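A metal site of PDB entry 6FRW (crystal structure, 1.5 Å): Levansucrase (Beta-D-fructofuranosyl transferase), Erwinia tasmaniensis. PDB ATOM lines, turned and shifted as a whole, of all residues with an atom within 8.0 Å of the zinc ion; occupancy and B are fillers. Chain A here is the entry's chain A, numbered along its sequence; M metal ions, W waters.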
ATOM      1  N   ARG A  47     -13.371   5.535  12.114  1.00  0.00           N
ATOM      2  CA  ARG A  47     -14.481   5.283  11.207  1.00  0.00           C
ATOM      3  C   ARG A  47     -15.702   4.843  11.999  1.00  0.00           C
ATOM      4  O   ARG A  47     -15.625   4.524  13.194  1.00  0.00           O
ATOM      5  CB  ARG A  47     -14.103   4.215  10.167  1.00  0.00           C
ATOM      6  CG  ARG A  47     -13.418   2.974  10.749  1.00  0.00           C
ATOM      7  CD  ARG A  47     -13.539   1.758   9.819  1.00  0.00           C
ATOM      8  NE  ARG A  47     -14.879   1.190   9.888  1.00  0.00           N
ATOM      9  CZ  ARG A  47     -15.179  -0.106   9.822  1.00  0.00           C
ATOM     10  NH1 ARG A  47     -16.452  -0.494   9.898  1.00  0.00           N
ATOM     11  NH2 ARG A  47     -14.220  -1.025   9.684  1.00  0.00           N
ATOM     12  N   ASP A  48     -16.851   4.799  11.318  1.00  0.00           N
ATOM     13  CA  ASP A  48     -18.072   4.262  11.888  1.00  0.00           C
ATOM     14  C   ASP A  48     -18.297   2.838  11.375  1.00  0.00           C
ATOM     15  O   ASP A  48     -17.457   2.267  10.688  1.00  0.00           O
ATOM     16  CB  ASP A  48     -19.275   5.175  11.592  1.00  0.00           C
ATOM     17  CG  ASP A  48     -19.590   5.293  10.108  1.00  0.00           C
ATOM     18  OD1 ASP A  48     -19.246   4.397   9.314  1.00  0.00           O
ATOM     19  OD2 ASP A  48     -20.191   6.319   9.742  1.00  0.00           O
ATOM     20  N   PHE A  49     -19.445   2.254  11.745  1.00  0.00           N
ATOM     21  CA  PHE A  49     -19.626   0.820  11.512  1.00  0.00           C
ATOM     22  C   PHE A  49     -19.848   0.448  10.046  1.00  0.00           C
ATOM     23  O   PHE A  49     -19.905  -0.744   9.754  1.00  0.00           O
ATOM     24  CB  PHE A  49     -20.783   0.295  12.363  1.00  0.00           C
ATOM     25  CG  PHE A  49     -20.367  -0.134  13.744  1.00  0.00           C
ATOM     26  CD1 PHE A  49     -19.517  -1.211  13.924  1.00  0.00           C
ATOM     27  CD2 PHE A  49     -20.831   0.533  14.859  1.00  0.00           C
ATOM     28  CE1 PHE A  49     -19.129  -1.614  15.194  1.00  0.00           C
ATOM     29  CE2 PHE A  49     -20.464   0.140  16.138  1.00  0.00           C
ATOM     30  CZ  PHE A  49     -19.616  -0.939  16.304  1.00  0.00           C
ATOM     31  N   ASP A  50     -19.936   1.395   9.118  1.00  0.00           N
ATOM     32  CA  ASP A  50     -20.035   1.052   7.698  1.00  0.00           C
ATOM     33  C   ASP A  50     -18.772   1.320   6.901  1.00  0.00           C
ATOM     34  O   ASP A  50     -18.662   0.807   5.769  1.00  0.00           O
ATOM     35  CB  ASP A  50     -21.190   1.821   7.037  1.00  0.00           C
ATOM     36  CG  ASP A  50     -20.957   3.318   7.012  1.00  0.00           C
ATOM     37  OD1 ASP A  50     -20.016   3.765   6.304  1.00  0.00           O
ATOM     38  OD2 ASP A  50     -21.712   4.046   7.686  1.00  0.00           O
ATOM     39  N   GLY A  51     -17.837   2.094   7.429  1.00  0.00           N
ATOM     40  CA  GLY A  51     -16.602   2.346   6.713  1.00  0.00           C
ATOM     41  C   GLY A  51     -16.271   3.820   6.588  1.00  0.00           C
ATOM     42  O   GLY A  51     -15.111   4.178   6.361  1.00  0.00           O
ATOM     43  N   ASP A  52     -17.286   4.672   6.721  1.00  0.00           N
ATOM     44  CA  ASP A  52     -17.086   6.110   6.619  1.00  0.00           C
ATOM     45  C   ASP A  52     -16.003   6.587   7.584  1.00  0.00           C
ATOM     46  O   ASP A  52     -16.051   6.288   8.774  1.00  0.00           O
ATOM     47  CB  ASP A  52     -18.380   6.858   6.941  1.00  0.00           C
ATOM     48  CG  ASP A  52     -19.358   6.860   5.780  1.00  0.00           C
ATOM     49  OD1 ASP A  52     -20.548   7.148   6.023  1.00  0.00           O
ATOM     50  OD2 ASP A  52     -18.948   6.563   4.644  1.00  0.00           O
ATOM     51  N   ILE A  53     -15.050   7.336   7.049  1.00  0.00           N
ATOM     52  CA  ILE A  53     -14.074   8.028   7.903  1.00  0.00           C
ATOM     53  C   ILE A  53     -14.751   9.227   8.548  1.00  0.00           C
ATOM     54  O   ILE A  53     -15.384  10.044   7.882  1.00  0.00           O
ATOM     55  CB  ILE A  53     -12.851   8.451   7.079  1.00  0.00           C
ATOM     56  CG1 ILE A  53     -12.322   7.264   6.251  1.00  0.00           C
ATOM     57  CG2 ILE A  53     -11.783   9.026   7.980  1.00  0.00           C
ATOM     58  CD1 ILE A  53     -12.195   5.963   7.038  1.00  0.00           C
ATOM     59  N   VAL A  54     -14.625   9.348   9.873  1.00  0.00           N
ATOM     60  CA  VAL A  54     -15.351  10.368  10.610  1.00  0.00           C
ATOM     61  C   VAL A  54     -14.362  11.236  11.372  1.00  0.00           C
ATOM     62  O   VAL A  54     -13.420  10.738  11.988  1.00  0.00           O
ATOM     63  CB  VAL A  54     -16.382   9.743  11.578  1.00  0.00           C
ATOM     64  CG1 VAL A  54     -17.437   8.987  10.788  1.00  0.00           C
ATOM     65  CG2 VAL A  54     -15.716   8.829  12.605  1.00  0.00           C
ATOM     66  N   LYS A 206     -26.523  -3.686   6.921  1.00  0.00           N
ATOM     67  CA  LYS A 206     -27.892  -3.213   7.082  1.00  0.00           C
ATOM     68  C   LYS A 206     -28.906  -4.195   6.518  1.00  0.00           C
ATOM     69  O   LYS A 206     -30.095  -4.096   6.840  1.00  0.00           O
ATOM     70  CB  LYS A 206     -28.057  -1.838   6.417  1.00  0.00           C
ATOM     71  CG  LYS A 206     -27.371  -0.690   7.155  1.00  0.00           C
ATOM     72  CD  LYS A 206     -27.712   0.645   6.508  1.00  0.00           C
ATOM     73  CE  LYS A 206     -26.884   1.788   7.075  1.00  0.00           C
ATOM     74  NZ  LYS A 206     -26.960   1.905   8.553  1.00  0.00           N
ATOM     75  N   PRO A 354     -13.845   4.417   1.627  1.00  0.00           N
ATOM     76  CA  PRO A 354     -15.002   4.481   0.725  1.00  0.00           C
ATOM     77  C   PRO A 354     -15.044   5.716  -0.165  1.00  0.00           C
ATOM     78  O   PRO A 354     -15.821   5.735  -1.122  1.00  0.00           O
ATOM     79  CB  PRO A 354     -16.210   4.453   1.673  1.00  0.00           C
ATOM     80  CG  PRO A 354     -15.686   3.908   2.951  1.00  0.00           C
ATOM     81  CD  PRO A 354     -14.278   4.382   3.045  1.00  0.00           C
ATOM     82  N   MET A 405     -14.844  11.819   5.826  1.00  0.00           N
ATOM     83  CA  MET A 405     -15.980  11.862   4.918  1.00  0.00           C
ATOM     84  C   MET A 405     -17.183  12.565   5.535  1.00  0.00           C
ATOM     85  O   MET A 405     -17.991  13.151   4.803  1.00  0.00           O
ATOM     86  CB  MET A 405     -16.366  10.448   4.511  1.00  0.00           C
ATOM     87  CG  MET A 405     -15.269   9.784   3.676  1.00  0.00           C
ATOM     88  SD  MET A 405     -15.481   8.016   3.522  1.00  0.00           S
ATOM     89  CE  MET A 405     -17.105   7.970   2.761  1.00  0.00           C
ATOM     90  N   LYS A 406     -17.303  12.501   6.847  1.00  0.00           N
ATOM     91  CA  LYS A 406     -18.345  13.217   7.566  1.00  0.00           C
ATOM     92  C   LYS A 406     -17.801  13.651   8.918  1.00  0.00           C
ATOM     93  O   LYS A 406     -16.869  13.055   9.455  1.00  0.00           O
ATOM     94  CB  LYS A 406     -19.601  12.351   7.752  1.00  0.00           C
ATOM     95  CG  LYS A 406     -19.360  11.109   8.587  1.00  0.00           C
ATOM     96  CD  LYS A 406     -20.567  10.180   8.595  1.00  0.00           C
ATOM     97  CE  LYS A 406     -21.827  10.912   8.981  1.00  0.00           C
ATOM     98  NZ  LYS A 406     -22.864   9.986   9.532  1.00  0.00           N
ATOM     99  N   ILE A 408     -18.729  14.527  12.930  1.00  0.00           N
ATOM    100  CA  ILE A 408     -19.659  14.220  14.009  1.00  0.00           C
ATOM    101  C   ILE A 408     -19.487  15.293  15.072  1.00  0.00           C
ATOM    102  O   ILE A 408     -18.394  15.471  15.630  1.00  0.00           O
ATOM    103  CB  ILE A 408     -19.408  12.823  14.590  1.00  0.00           C
ATOM    104  CG1 ILE A 408     -19.477  11.752  13.502  1.00  0.00           C
ATOM    105  CG2 ILE A 408     -20.385  12.513  15.722  1.00  0.00           C
ATOM    106  CD1 ILE A 408     -20.839  11.630  12.816  1.00  0.00           C
HETATM  107 ZN    ZN M   1     -21.397   6.071   7.948  1.00  0.00          ZN
HETATM  108  O   HOH W   1     -23.473   7.035   8.320  1.00  0.00           O
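OD1 of Asp 48 sits at hydrogen-bond distance from N of Gly 51 (3.3 Å).
Three residues have an atom within 4 Å of the zinc ion: Asp 48, Asp 50 and Asp 52. The nearest printed residue that does not touch the zinc ion is Lys 406 (4.2 Å).
The zinc ion is bound by OD2 of Asp 50 (2.1 Å), OD2 of Asp 48 (2.2 Å), water W1 (2.3 Å) and OD1 of Asp 52 (2.4 Å).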
